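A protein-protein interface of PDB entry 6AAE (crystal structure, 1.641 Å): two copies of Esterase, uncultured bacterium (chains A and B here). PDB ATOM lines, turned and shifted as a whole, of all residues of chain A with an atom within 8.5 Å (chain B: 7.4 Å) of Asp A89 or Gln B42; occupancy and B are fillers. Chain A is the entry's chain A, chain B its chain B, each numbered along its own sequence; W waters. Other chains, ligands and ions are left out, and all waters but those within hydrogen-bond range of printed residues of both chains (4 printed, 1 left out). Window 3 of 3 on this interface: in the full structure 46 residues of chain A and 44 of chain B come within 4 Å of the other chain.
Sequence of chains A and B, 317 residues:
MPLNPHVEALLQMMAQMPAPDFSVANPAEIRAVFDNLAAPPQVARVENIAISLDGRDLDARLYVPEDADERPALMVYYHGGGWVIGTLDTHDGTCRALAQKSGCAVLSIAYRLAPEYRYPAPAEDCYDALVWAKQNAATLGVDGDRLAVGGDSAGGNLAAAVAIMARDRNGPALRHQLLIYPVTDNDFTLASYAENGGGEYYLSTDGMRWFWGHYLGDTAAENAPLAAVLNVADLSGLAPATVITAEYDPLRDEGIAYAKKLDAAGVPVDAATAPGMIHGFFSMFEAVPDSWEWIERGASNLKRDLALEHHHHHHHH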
ATOM      1  N   VAL A  46      -0.108  -3.635  27.431  1.00  0.00           N
ATOM      2  CA  VAL A  46       0.162  -2.448  26.650  1.00  0.00           C
ATOM      3  C   VAL A  46      -1.157  -1.716  26.526  1.00  0.00           C
ATOM      4  O   VAL A  46      -2.158  -2.318  26.147  1.00  0.00           O
ATOM      5  CB  VAL A  46       0.711  -2.776  25.261  1.00  0.00           C
ATOM      6  CG1 VAL A  46       1.016  -1.501  24.500  1.00  0.00           C
ATOM      7  CG2 VAL A  46       1.959  -3.628  25.377  1.00  0.00           C
ATOM      8  N   ASN A  48      -3.015   1.841  24.996  1.00  0.00           N
ATOM      9  CA  ASN A  48      -2.992   3.073  24.234  1.00  0.00           C
ATOM     10  C   ASN A  48      -3.745   4.147  24.992  1.00  0.00           C
ATOM     11  O   ASN A  48      -4.912   3.979  25.334  1.00  0.00           O
ATOM     12  CB  ASN A  48      -3.597   2.859  22.849  1.00  0.00           C
ATOM     13  CG  ASN A  48      -2.681   2.080  21.940  1.00  0.00           C
ATOM     14  OD1 ASN A  48      -1.467   2.291  21.949  1.00  0.00           O
ATOM     15  ND2 ASN A  48      -3.246   1.162  21.157  1.00  0.00           N
ATOM     16  N   ASP A  59      -0.886  11.290  21.707  1.00  0.00           N
ATOM     17  CA  ASP A  59      -0.984   9.846  21.860  1.00  0.00           C
ATOM     18  C   ASP A  59       0.138   9.377  22.767  1.00  0.00           C
ATOM     19  O   ASP A  59       1.243   9.914  22.705  1.00  0.00           O
ATOM     20  CB  ASP A  59      -0.897   9.146  20.507  1.00  0.00           C
ATOM     21  CG  ASP A  59      -2.117   9.391  19.638  1.00  0.00           C
ATOM     22  OD1 ASP A  59      -3.226   9.549  20.187  1.00  0.00           O
ATOM     23  OD2 ASP A  59      -1.963   9.427  18.399  1.00  0.00           O
ATOM     24  N   ARG A  61       1.635   5.532  25.026  1.00  0.00           N
ATOM     25  CA  ARG A  61       1.478   4.102  25.192  1.00  0.00           C
ATOM     26  C   ARG A  61       2.164   3.679  26.473  1.00  0.00           C
ATOM     27  O   ARG A  61       3.321   4.022  26.717  1.00  0.00           O
ATOM     28  CB  ARG A  61       2.039   3.346  23.985  1.00  0.00           C
ATOM     29  CG  ARG A  61       1.519   1.946  23.816  1.00  0.00           C
ATOM     30  CD  ARG A  61       1.943   1.352  22.468  1.00  0.00           C
ATOM     31  NE  ARG A  61       1.206   1.909  21.332  1.00  0.00           N
ATOM     32  CZ  ARG A  61       1.562   1.746  20.059  1.00  0.00           C
ATOM     33  NH1 ARG A  61       2.651   1.050  19.749  1.00  0.00           N
ATOM     34  NH2 ARG A  61       0.839   2.277  19.089  1.00  0.00           N
ATOM     35  N   TYR A  63       3.449   0.658  28.892  1.00  0.00           N
ATOM     36  CA  TYR A  63       3.910  -0.719  28.876  1.00  0.00           C
ATOM     37  C   TYR A  63       4.117  -1.155  30.320  1.00  0.00           C
ATOM     38  O   TYR A  63       4.843  -0.505  31.067  1.00  0.00           O
ATOM     39  CB  TYR A  63       5.229  -0.862  28.103  1.00  0.00           C
ATOM     40  CG  TYR A  63       5.200  -0.347  26.685  1.00  0.00           C
ATOM     41  CD1 TYR A  63       5.331   1.019  26.415  1.00  0.00           C
ATOM     42  CD2 TYR A  63       5.043  -1.226  25.611  1.00  0.00           C
ATOM     43  CE1 TYR A  63       5.308   1.491  25.107  1.00  0.00           C
ATOM     44  CE2 TYR A  63       5.016  -0.762  24.309  1.00  0.00           C
ATOM     45  CZ  TYR A  63       5.147   0.598  24.067  1.00  0.00           C
ATOM     46  OH  TYR A  63       5.124   1.057  22.761  1.00  0.00           O
ATOM     47  N   HIS A  79      10.683   8.939  22.037  1.00  0.00           N
ATOM     48  CA  HIS A  79      11.284   8.279  20.874  1.00  0.00           C
ATOM     49  C   HIS A  79      12.233   9.189  20.109  1.00  0.00           C
ATOM     50  O   HIS A  79      12.093  10.407  20.115  1.00  0.00           O
ATOM     51  CB  HIS A  79      10.207   7.779  19.909  1.00  0.00           C
ATOM     52  CG  HIS A  79       9.458   8.869  19.204  1.00  0.00           C
ATOM     53  ND1 HIS A  79       9.924   9.468  18.053  1.00  0.00           N
ATOM     54  CD2 HIS A  79       8.263   9.450  19.472  1.00  0.00           C
ATOM     55  CE1 HIS A  79       9.052  10.372  17.641  1.00  0.00           C
ATOM     56  NE2 HIS A  79       8.031  10.379  18.483  1.00  0.00           N
ATOM     57  N   GLY A  86       9.550   9.383  13.397  1.00  0.00           N
ATOM     58  CA  GLY A  86       9.374   8.479  14.524  1.00  0.00           C
ATOM     59  C   GLY A  86       7.956   8.500  15.058  1.00  0.00           C
ATOM     60  O   GLY A  86       7.273   9.527  15.000  1.00  0.00           O
ATOM     61  N   THR A  87       7.519   7.360  15.592  1.00  0.00           N
ATOM     62  CA  THR A  87       6.166   7.201  16.124  1.00  0.00           C
ATOM     63  C   THR A  87       6.176   6.269  17.324  1.00  0.00           C
ATOM     64  O   THR A  87       7.192   5.660  17.652  1.00  0.00           O
ATOM     65  CB  THR A  87       5.198   6.601  15.081  1.00  0.00           C
ATOM     66  OG1 THR A  87       5.613   5.259  14.786  1.00  0.00           O
ATOM     67  CG2 THR A  87       5.158   7.426  13.783  1.00  0.00           C
ATOM     68  N   LEU A  88       5.021   6.112  17.962  1.00  0.00           N
ATOM     69  CA  LEU A  88       4.912   5.094  19.008  1.00  0.00           C
ATOM     70  C   LEU A  88       5.214   3.707  18.463  1.00  0.00           C
ATOM     71  O   LEU A  88       5.800   2.882  19.153  1.00  0.00           O
ATOM     72  CB  LEU A  88       3.521   5.095  19.638  1.00  0.00           C
ATOM     73  CG  LEU A  88       3.135   6.406  20.313  1.00  0.00           C
ATOM     74  CD1 LEU A  88       1.741   6.291  20.901  1.00  0.00           C
ATOM     75  CD2 LEU A  88       4.140   6.762  21.385  1.00  0.00           C
ATOM     76  N   ASP A  89       4.821   3.457  17.222  1.00  0.00           N
ATOM     77  CA  ASP A  89       5.057   2.154  16.605  1.00  0.00           C
ATOM     78  C   ASP A  89       6.527   1.921  16.240  1.00  0.00           C
ATOM     79  O   ASP A  89       7.023   0.804  16.387  1.00  0.00           O
ATOM     80  CB  ASP A  89       4.176   1.993  15.365  1.00  0.00           C
ATOM     81  CG  ASP A  89       2.709   1.764  15.722  1.00  0.00           C
ATOM     82  OD1 ASP A  89       2.441   1.033  16.697  1.00  0.00           O
ATOM     83  OD2 ASP A  89       1.834   2.319  15.031  1.00  0.00           O
ATOM     84  N   THR A  90       7.247   2.950  15.785  1.00  0.00           N
ATOM     85  CA  THR A  90       8.648   2.702  15.427  1.00  0.00           C
ATOM     86  C   THR A  90       9.466   2.313  16.656  1.00  0.00           C
ATOM     87  O   THR A  90      10.432   1.548  16.554  1.00  0.00           O
ATOM     88  CB  THR A  90       9.320   3.911  14.742  1.00  0.00           C
ATOM     89  OG1 THR A  90       9.319   5.039  15.621  1.00  0.00           O
ATOM     90  CG2 THR A  90       8.610   4.271  13.432  1.00  0.00           C
ATOM     91  N   HIS A  91       9.052   2.794  17.823  1.00  0.00           N
ATOM     92  CA  HIS A  91       9.814   2.550  19.042  1.00  0.00           C
ATOM     93  C   HIS A  91       9.129   1.612  20.021  1.00  0.00           C
ATOM     94  O   HIS A  91       9.574   1.466  21.153  1.00  0.00           O
ATOM     95  CB  HIS A  91      10.142   3.878  19.711  1.00  0.00           C
ATOM     96  CG  HIS A  91      11.276   4.585  19.043  1.00  0.00           C
ATOM     97  ND1 HIS A  91      11.194   5.048  17.747  1.00  0.00           N
ATOM     98  CD2 HIS A  91      12.539   4.835  19.456  1.00  0.00           C
ATOM     99  CE1 HIS A  91      12.352   5.582  17.398  1.00  0.00           C
ATOM    100  NE2 HIS A  91      13.188   5.467  18.419  1.00  0.00           N
ATOM    101  N   ASP A  92       8.079   0.942  19.556  1.00  0.00           N
ATOM    102  CA  ASP A  92       7.336   0.009  20.403  1.00  0.00           C
ATOM    103  C   ASP A  92       8.229  -1.131  20.905  1.00  0.00           C
ATOM    104  O   ASP A  92       8.205  -1.476  22.084  1.00  0.00           O
ATOM    105  CB  ASP A  92       6.143  -0.550  19.624  1.00  0.00           C
ATOM    106  CG  ASP A  92       5.253  -1.442  20.468  1.00  0.00           C
ATOM    107  OD1 ASP A  92       4.337  -0.902  21.130  1.00  0.00           O
ATOM    108  OD2 ASP A  92       5.453  -2.679  20.434  1.00  0.00           O
ATOM    109  N   GLY A  93       9.020  -1.721  20.018  1.00  0.00           N
ATOM    110  CA  GLY A  93       9.901  -2.810  20.428  1.00  0.00           C
ATOM    111  C   GLY A  93      10.933  -2.359  21.451  1.00  0.00           C
ATOM    112  O   GLY A  93      11.202  -3.041  22.433  1.00  0.00           O
ATOM    113  N   THR A  94      11.499  -1.184  21.222  1.00  0.00           N
ATOM    114  CA  THR A  94      12.475  -0.594  22.146  1.00  0.00           C
ATOM    115  C   THR A  94      11.884  -0.369  23.541  1.00  0.00           C
ATOM    116  O   THR A  94      12.495  -0.720  24.557  1.00  0.00           O
ATOM    117  CB  THR A  94      13.003   0.742  21.587  1.00  0.00           C
ATOM    118  OG1 THR A  94      13.560   0.523  20.281  1.00  0.00           O
ATOM    119  CG2 THR A  94      14.047   1.327  22.501  1.00  0.00           C
ATOM    120  N   CYS A  95      10.679   0.187  23.599  1.00  0.00           N
ATOM    121  CA  CYS A  95      10.015   0.365  24.890  1.00  0.00           C
ATOM    122  C   CYS A  95       9.678  -0.960  25.587  1.00  0.00           C
ATOM    123  O   CYS A  95       9.856  -1.068  26.787  1.00  0.00           O
ATOM    124  CB  CYS A  95       8.745   1.196  24.724  1.00  0.00           C
ATOM    125  SG  CYS A  95       9.101   2.893  24.295  1.00  0.00           S
ATOM    126  N   ARG A  96       9.211  -1.961  24.836  1.00  0.00           N
ATOM    127  CA  ARG A  96       8.944  -3.285  25.410  1.00  0.00           C
ATOM    128  C   ARG A  96      10.215  -3.868  26.009  1.00  0.00           C
ATOM    129  O   ARG A  96      10.203  -4.425  27.108  1.00  0.00           O
ATOM    130  CB  ARG A  96       8.394  -4.251  24.357  1.00  0.00           C
ATOM    131  CG  ARG A  96       6.987  -3.911  23.873  1.00  0.00           C
ATOM    132  CD  ARG A  96       6.660  -4.666  22.595  1.00  0.00           C
ATOM    133  NE  ARG A  96       5.238  -4.610  22.279  1.00  0.00           N
ATOM    134  CZ  ARG A  96       4.353  -5.482  22.755  1.00  0.00           C
ATOM    135  NH1 ARG A  96       4.756  -6.467  23.556  1.00  0.00           N
ATOM    136  NH2 ARG A  96       3.073  -5.382  22.431  1.00  0.00           N
ATOM    137  N   SER A 108       5.451   5.790  26.762  1.00  0.00           N
ATOM    138  CA  SER A 108       6.001   6.385  25.549  1.00  0.00           C
ATOM    139  C   SER A 108       5.115   7.527  25.026  1.00  0.00           C
ATOM    140  O   SER A 108       3.907   7.368  24.868  1.00  0.00           O
ATOM    141  CB  SER A 108       6.187   5.295  24.485  1.00  0.00           C
ATOM    142  OG  SER A 108       6.855   5.814  23.348  1.00  0.00           O
ATOM    143  N   ALA A 110       4.038  10.451  22.226  1.00  0.00           N
ATOM    144  CA  ALA A 110       4.096  10.960  20.855  1.00  0.00           C
ATOM    145  C   ALA A 110       4.004  12.482  20.872  1.00  0.00           C
ATOM    146  O   ALA A 110       2.939  13.059  20.639  1.00  0.00           O
ATOM    147  CB  ALA A 110       2.987  10.366  20.005  1.00  0.00           C
ATOM    148  N   ASP B  35       9.048   5.704   8.873  1.00  0.00           N
ATOM    149  CA  ASP B  35       8.106   5.221   9.870  1.00  0.00           C
ATOM    150  C   ASP B  35       7.602   3.843   9.456  1.00  0.00           C
ATOM    151  O   ASP B  35       7.146   3.071  10.293  1.00  0.00           O
ATOM    152  CB  ASP B  35       6.948   6.217  10.076  1.00  0.00           C
ATOM    153  CG  ASP B  35       7.404   7.549  10.719  1.00  0.00           C
ATOM    154  OD1 ASP B  35       8.517   7.625  11.272  1.00  0.00           O
ATOM    155  OD2 ASP B  35       6.634   8.532  10.678  1.00  0.00           O
ATOM    156  N   ASN B  36       7.746   3.513   8.174  1.00  0.00           N
ATOM    157  CA  ASN B  36       7.248   2.243   7.645  1.00  0.00           C
ATOM    158  C   ASN B  36       8.305   1.192   7.343  1.00  0.00           C
ATOM    159  O   ASN B  36       8.005   0.147   6.776  1.00  0.00           O
ATOM    160  CB  ASN B  36       6.433   2.500   6.387  1.00  0.00           C
ATOM    161  CG  ASN B  36       5.011   2.866   6.701  1.00  0.00           C
ATOM    162  OD1 ASN B  36       4.325   2.137   7.422  1.00  0.00           O
ATOM    163  ND2 ASN B  36       4.559   4.010   6.192  1.00  0.00           N
ATOM    164  N   ALA B  38      11.180  -1.322   9.182  1.00  0.00           N
ATOM    165  CA  ALA B  38      11.485  -1.935  10.478  1.00  0.00           C
ATOM    166  C   ALA B  38      10.472  -1.584  11.580  1.00  0.00           C
ATOM    167  O   ALA B  38      10.836  -1.479  12.755  1.00  0.00           O
ATOM    168  CB  ALA B  38      12.888  -1.543  10.925  1.00  0.00           C
ATOM    169  N   ALA B  39       9.209  -1.407  11.204  1.00  0.00           N
ATOM    170  CA  ALA B  39       8.173  -1.085  12.177  1.00  0.00           C
ATOM    171  C   ALA B  39       6.816  -1.602  11.730  1.00  0.00           C
ATOM    172  O   ALA B  39       6.442  -1.421  10.577  1.00  0.00           O
ATOM    173  CB  ALA B  39       8.107   0.414  12.400  1.00  0.00           C
ATOM    174  N   PRO B  40       6.055  -2.201  12.660  1.00  0.00           N
ATOM    175  CA  PRO B  40       4.708  -2.667  12.328  1.00  0.00           C
ATOM    176  C   PRO B  40       3.849  -1.515  11.809  1.00  0.00           C
ATOM    177  O   PRO B  40       3.951  -0.404  12.299  1.00  0.00           O
ATOM    178  CB  PRO B  40       4.178  -3.190  13.665  1.00  0.00           C
ATOM    179  CG  PRO B  40       4.886  -2.369  14.690  1.00  0.00           C
ATOM    180  CD  PRO B  40       6.273  -2.135  14.119  1.00  0.00           C
ATOM    181  N   PRO B  41       3.018  -1.782  10.803  1.00  0.00           N
ATOM    182  CA  PRO B  41       2.181  -0.759  10.172  1.00  0.00           C
ATOM    183  C   PRO B  41       1.251  -0.082  11.183  1.00  0.00           C
ATOM    184  O   PRO B  41       0.695  -0.741  12.065  1.00  0.00           O
ATOM    185  CB  PRO B  41       1.387  -1.562   9.134  1.00  0.00           C
ATOM    186  CG  PRO B  41       2.239  -2.749   8.862  1.00  0.00           C
ATOM    187  CD  PRO B  41       2.862  -3.100  10.168  1.00  0.00           C
ATOM    188  N   GLN B  42       1.101   1.232  11.065  1.00  0.00           N
ATOM    189  CA  GLN B  42       0.219   1.973  11.952  1.00  0.00           C
ATOM    190  C   GLN B  42      -1.257   1.673  11.664  1.00  0.00           C
ATOM    191  O   GLN B  42      -1.664   1.589  10.507  1.00  0.00           O
ATOM    192  CB  GLN B  42       0.492   3.468  11.807  1.00  0.00           C
ATOM    193  CG  GLN B  42      -0.169   4.342  12.846  1.00  0.00           C
ATOM    194  CD  GLN B  42       0.331   5.777  12.778  1.00  0.00           C
ATOM    195  OE1 GLN B  42       1.542   6.028  12.737  1.00  0.00           O
ATOM    196  NE2 GLN B  42      -0.601   6.727  12.756  1.00  0.00           N
ATOM    197  N   VAL B  43      -2.051   1.498  12.718  1.00  0.00           N
ATOM    198  CA  VAL B  43      -3.508   1.410  12.566  1.00  0.00           C
ATOM    199  C   VAL B  43      -4.137   2.351  13.591  1.00  0.00           C
ATOM    200  O   VAL B  43      -3.471   2.779  14.523  1.00  0.00           O
ATOM    201  CB  VAL B  43      -4.027  -0.022  12.755  1.00  0.00           C
ATOM    202  CG1 VAL B  43      -3.438  -0.954  11.689  1.00  0.00           C
ATOM    203  CG2 VAL B  43      -3.665  -0.496  14.108  1.00  0.00           C
ATOM    204  N   ALA B  44      -5.404   2.702  13.407  1.00  0.00           N
ATOM    205  CA  ALA B  44      -6.043   3.705  14.262  1.00  0.00           C
ATOM    206  C   ALA B  44      -6.360   3.197  15.667  1.00  0.00           C
ATOM    207  O   ALA B  44      -6.150   3.891  16.664  1.00  0.00           O
ATOM    208  CB  ALA B  44      -7.319   4.203  13.598  1.00  0.00           C
ATOM    209  N   ARG B  45      -6.906   1.992  15.740  1.00  0.00           N
ATOM    210  CA  ARG B  45      -7.305   1.396  17.009  1.00  0.00           C
ATOM    211  C   ARG B  45      -6.873  -0.058  17.054  1.00  0.00           C
ATOM    212  O   ARG B  45      -7.017  -0.775  16.072  1.00  0.00           O
ATOM    213  CB  ARG B  45      -8.820   1.468  17.207  1.00  0.00           C
ATOM    214  CG  ARG B  45      -9.359   2.821  17.589  1.00  0.00           C
ATOM    215  CD  ARG B  45     -10.533   2.672  18.548  1.00  0.00           C
ATOM    216  NE  ARG B  45     -11.395   1.540  18.212  1.00  0.00           N
ATOM    217  CZ  ARG B  45     -12.289   1.545  17.226  1.00  0.00           C
ATOM    218  NH1 ARG B  45     -13.038   0.470  17.006  1.00  0.00           N
ATOM    219  NH2 ARG B  45     -12.432   2.623  16.461  1.00  0.00           N
ATOM    220  N   VAL B  46      -6.324  -0.478  18.187  1.00  0.00           N
ATOM    221  CA  VAL B  46      -6.068  -1.890  18.441  1.00  0.00           C
ATOM    222  C   VAL B  46      -6.622  -2.202  19.813  1.00  0.00           C
ATOM    223  O   VAL B  46      -6.314  -1.511  20.769  1.00  0.00           O
ATOM    224  CB  VAL B  46      -4.572  -2.249  18.392  1.00  0.00           C
ATOM    225  CG1 VAL B  46      -4.366  -3.709  18.758  1.00  0.00           C
ATOM    226  CG2 VAL B  46      -4.015  -2.006  17.024  1.00  0.00           C
ATOM    227  N   VAL B  64      -8.482  -1.777  13.797  1.00  0.00           N
ATOM    228  CA  VAL B  64      -9.279  -0.898  12.944  1.00  0.00           C
ATOM    229  C   VAL B  64      -8.350   0.118  12.296  1.00  0.00           C
ATOM    230  O   VAL B  64      -7.707   0.906  12.988  1.00  0.00           O
ATOM    231  CB  VAL B  64     -10.402  -0.187  13.735  1.00  0.00           C
ATOM    232  CG1 VAL B  64     -11.250   0.658  12.797  1.00  0.00           C
ATOM    233  CG2 VAL B  64     -11.279  -1.200  14.434  1.00  0.00           C
ATOM    234  N   PRO B  65      -8.236   0.070  10.959  1.00  0.00           N
ATOM    235  CA  PRO B  65      -7.296   0.932  10.245  1.00  0.00           C
ATOM    236  C   PRO B  65      -7.780   2.365  10.123  1.00  0.00           C
ATOM    237  O   PRO B  65      -8.968   2.651  10.290  1.00  0.00           O
ATOM    238  CB  PRO B  65      -7.204   0.278   8.864  1.00  0.00           C
ATOM    239  CG  PRO B  65      -8.535  -0.369   8.688  1.00  0.00           C
ATOM    240  CD  PRO B  65      -8.931  -0.861  10.050  1.00  0.00           C
ATOM    241  N   GLU B  66      -6.838   3.247   9.806  1.00  0.00           N
ATOM    242  CA  GLU B  66      -7.078   4.682   9.745  1.00  0.00           C
ATOM    243  C   GLU B  66      -8.320   5.085   8.943  1.00  0.00           C
ATOM    244  O   GLU B  66      -9.195   5.787   9.450  1.00  0.00           O
ATOM    245  CB  GLU B  66      -5.844   5.373   9.161  1.00  0.00           C
ATOM    246  CG  GLU B  66      -4.552   5.068   9.910  1.00  0.00           C
ATOM    247  CD  GLU B  66      -4.382   5.904  11.166  1.00  0.00           C
ATOM    248  OE1 GLU B  66      -5.314   6.669  11.515  1.00  0.00           O
ATOM    249  OE2 GLU B  66      -3.312   5.791  11.807  1.00  0.00           O
ATOM    250  N   ASP B  92       0.787 -10.226  14.930  1.00  0.00           N
ATOM    251  CA  ASP B  92       0.290  -8.866  15.059  1.00  0.00           C
ATOM    252  C   ASP B  92       0.729  -8.001  13.864  1.00  0.00           C
ATOM    253  O   ASP B  92      -0.073  -7.221  13.323  1.00  0.00           O
ATOM    254  CB  ASP B  92       0.772  -8.282  16.388  1.00  0.00           C
ATOM    255  CG  ASP B  92       0.271  -6.880  16.631  1.00  0.00           C
ATOM    256  OD1 ASP B  92      -0.853  -6.741  17.162  1.00  0.00           O
ATOM    257  OD2 ASP B  92       1.018  -5.933  16.307  1.00  0.00           O
ATOM    258  N   ARG B  96      -1.776  -6.146  11.137  1.00  0.00           N
ATOM    259  CA  ARG B  96      -1.719  -4.696  10.940  1.00  0.00           C
ATOM    260  C   ARG B  96      -1.576  -4.392   9.454  1.00  0.00           C
ATOM    261  O   ARG B  96      -2.235  -3.498   8.931  1.00  0.00           O
ATOM    262  CB  ARG B  96      -0.558  -4.069  11.715  1.00  0.00           C
ATOM    263  CG  ARG B  96      -0.767  -4.036  13.219  1.00  0.00           C
ATOM    264  CD  ARG B  96       0.529  -3.672  13.915  1.00  0.00           C
ATOM    265  NE  ARG B  96       0.288  -3.398  15.324  1.00  0.00           N
ATOM    266  CZ  ARG B  96      -0.059  -2.208  15.795  1.00  0.00           C
ATOM    267  NH1 ARG B  96      -0.171  -1.180  14.966  1.00  0.00           N
ATOM    268  NH2 ARG B  96      -0.277  -2.041  17.095  1.00  0.00           N
ATOM    269  N   ALA B  97      -0.707  -5.141   8.783  1.00  0.00           N
ATOM    270  CA  ALA B  97      -0.462  -4.921   7.360  1.00  0.00           C
ATOM    271  C   ALA B  97      -1.734  -5.159   6.554  1.00  0.00           C
ATOM    272  O   ALA B  97      -2.066  -4.382   5.662  1.00  0.00           O
ATOM    273  CB  ALA B  97       0.661  -5.815   6.865  1.00  0.00           C
ATOM    274  N   ALA B  99      -4.880  -5.083   7.643  1.00  0.00           N
ATOM    275  CA  ALA B  99      -5.895  -4.068   7.957  1.00  0.00           C
ATOM    276  C   ALA B  99      -5.606  -2.767   7.208  1.00  0.00           C
ATOM    277  O   ALA B  99      -6.500  -2.171   6.580  1.00  0.00           O
ATOM    278  CB  ALA B  99      -5.953  -3.812   9.458  1.00  0.00           C
ATOM    279  N   GLN B 100      -4.353  -2.343   7.271  1.00  0.00           N
ATOM    280  CA  GLN B 100      -3.918  -1.091   6.653  1.00  0.00           C
ATOM    281  C   GLN B 100      -4.140  -1.094   5.140  1.00  0.00           C
ATOM    282  O   GLN B 100      -4.651  -0.127   4.569  1.00  0.00           O
ATOM    283  CB  GLN B 100      -2.444  -0.856   6.977  1.00  0.00           C
ATOM    284  CG  GLN B 100      -1.858   0.442   6.449  1.00  0.00           C
ATOM    285  CD  GLN B 100      -0.386   0.573   6.809  1.00  0.00           C
ATOM    286  OE1 GLN B 100       0.451  -0.191   6.328  1.00  0.00           O
ATOM    287  NE2 GLN B 100      -0.066   1.531   7.668  1.00  0.00           N
HETATM  288  O   HOH W   1       2.223   5.013  15.766  1.00  0.00           O
HETATM  289  O   HOH W   2      -5.926   1.604  20.353  1.00  0.00           O
HETATM  290  O   HOH W   3      -0.677   1.682  15.507  1.00  0.00           O
HETATM  291  O   HOH W   4       6.653  10.614  12.428  1.00  0.00           O
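NH1 of Arg B96 is in salt-bridge range of OD1 of Asp A89 (3.8 Å).
OD1 of Asp B35 lies within hydrogen-bond range of N of Gly A86.
The side-chain hydroxyl (OG1) of Thr A87 lies close to the backbone NH (N) of Asp A89 (3.1 Å).
The side-chain amide nitrogen of Gln B100 is in hydrogen-bond range of the backbone carbonyl oxygen of Gln B42, at 3.3 Å.
N of Thr A87 lies within hydrogen-bond range of OG1 of Thr A90, 2.9 Å away.
The side-chain carboxylate of Asp A89 lies within salt-bridge range of the guanidinium group of Arg A61.
O of Pro B41 lies within hydrogen-bond range of NH1 of Arg B96 (3.1 Å).
NE2 of Gln B42 is in hydrogen-bond range of OE2 of Glu B66.
Thr A87 touches Asp B35 (CG2 to OD2, 3.6 Å).
Pro B40 touches Asp A89 (CD to O, 3.8 Å).
CA of Gln B42 touches OD2 of Asp A89, at 3.5 Å.
Asp B35 touches Thr A90.
Ala B39 touches Thr A90 (CB to CA, 3.8 Å).
Printed residues of chain B within 4 Å of Thr A87: Asp B35 (3.6 Å).
Asp A89 touches three residues of chain B.
Of the printed residues of chain B, Thr A90 touches Asp B35 (3.7 Å) and Ala B39 (3.8 Å).
Of the printed residues of chain A, Asp B35 touches Gly A86 (2.9 Å), Thr A87 (3.6 Å) and Thr A90 (3.7 Å).
Of the printed residues of chain A, Ala B39 touches Thr A90 (3.8 Å).
Printed residues of chain A within 4 Å of Pro B40: Asp A89 (3.8 Å).
Of the printed residues of chain A, Gln B42 touches Asp A89.
Val B64 touches none of the printed residues of chain A.
The nearest residue of chain B that does not touch Asp A89 is Ala B39 (4.2 Å).
The nearest printed residue of chain A that does not touch Pro B40 is Asp A92 (5.4 Å).
Printed residues of chain B that touch a printed residue of chain A: Asp B35, Ala B39, Pro B40, Gln B42 and Arg B96.
Hydrophobic or aromatic side chains of chain B that line the printed part of chain A: Ala B39 and Pro B40.
Along chain A the printed residues that touch a printed residue of chain B span positions 86 to 90.
Among the printed residues, 7 pairs touch across the chains.
Among the printed residues, Asp or Glu carboxylates within 4 Å of a Lys or Arg side-chain nitrogen of the other chain: Asp A89 with Arg B96 (3.8 Å).
Positions printed for both chains: 46, 92 and 96.
Of the 7 pairs that touch across the chains among the printed residues, none has its exchanged pair printed and touching as well.
Water W3 lies within hydrogen-bond range of the side-chain carboxylate (OD2) of Asp A89 (2.6 Å), the guanidinium group (NH1) of Arg B96 (3.0 Å) and the backbone NH (N) of Val B43 (3.1 Å).
Water W4 lies within hydrogen-bond range of OD2 of Asp B35 (2.7 Å) and O of Gly A86 (2.9 Å).
Water W1 bridges OD2 of Asp A89 (2.8 Å) and OE1 of Gln B42 (3.3 Å).
Water W2 bridges ND2 of Asn A48 (2.8 Å) and N of Val B46 (3.0 Å).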
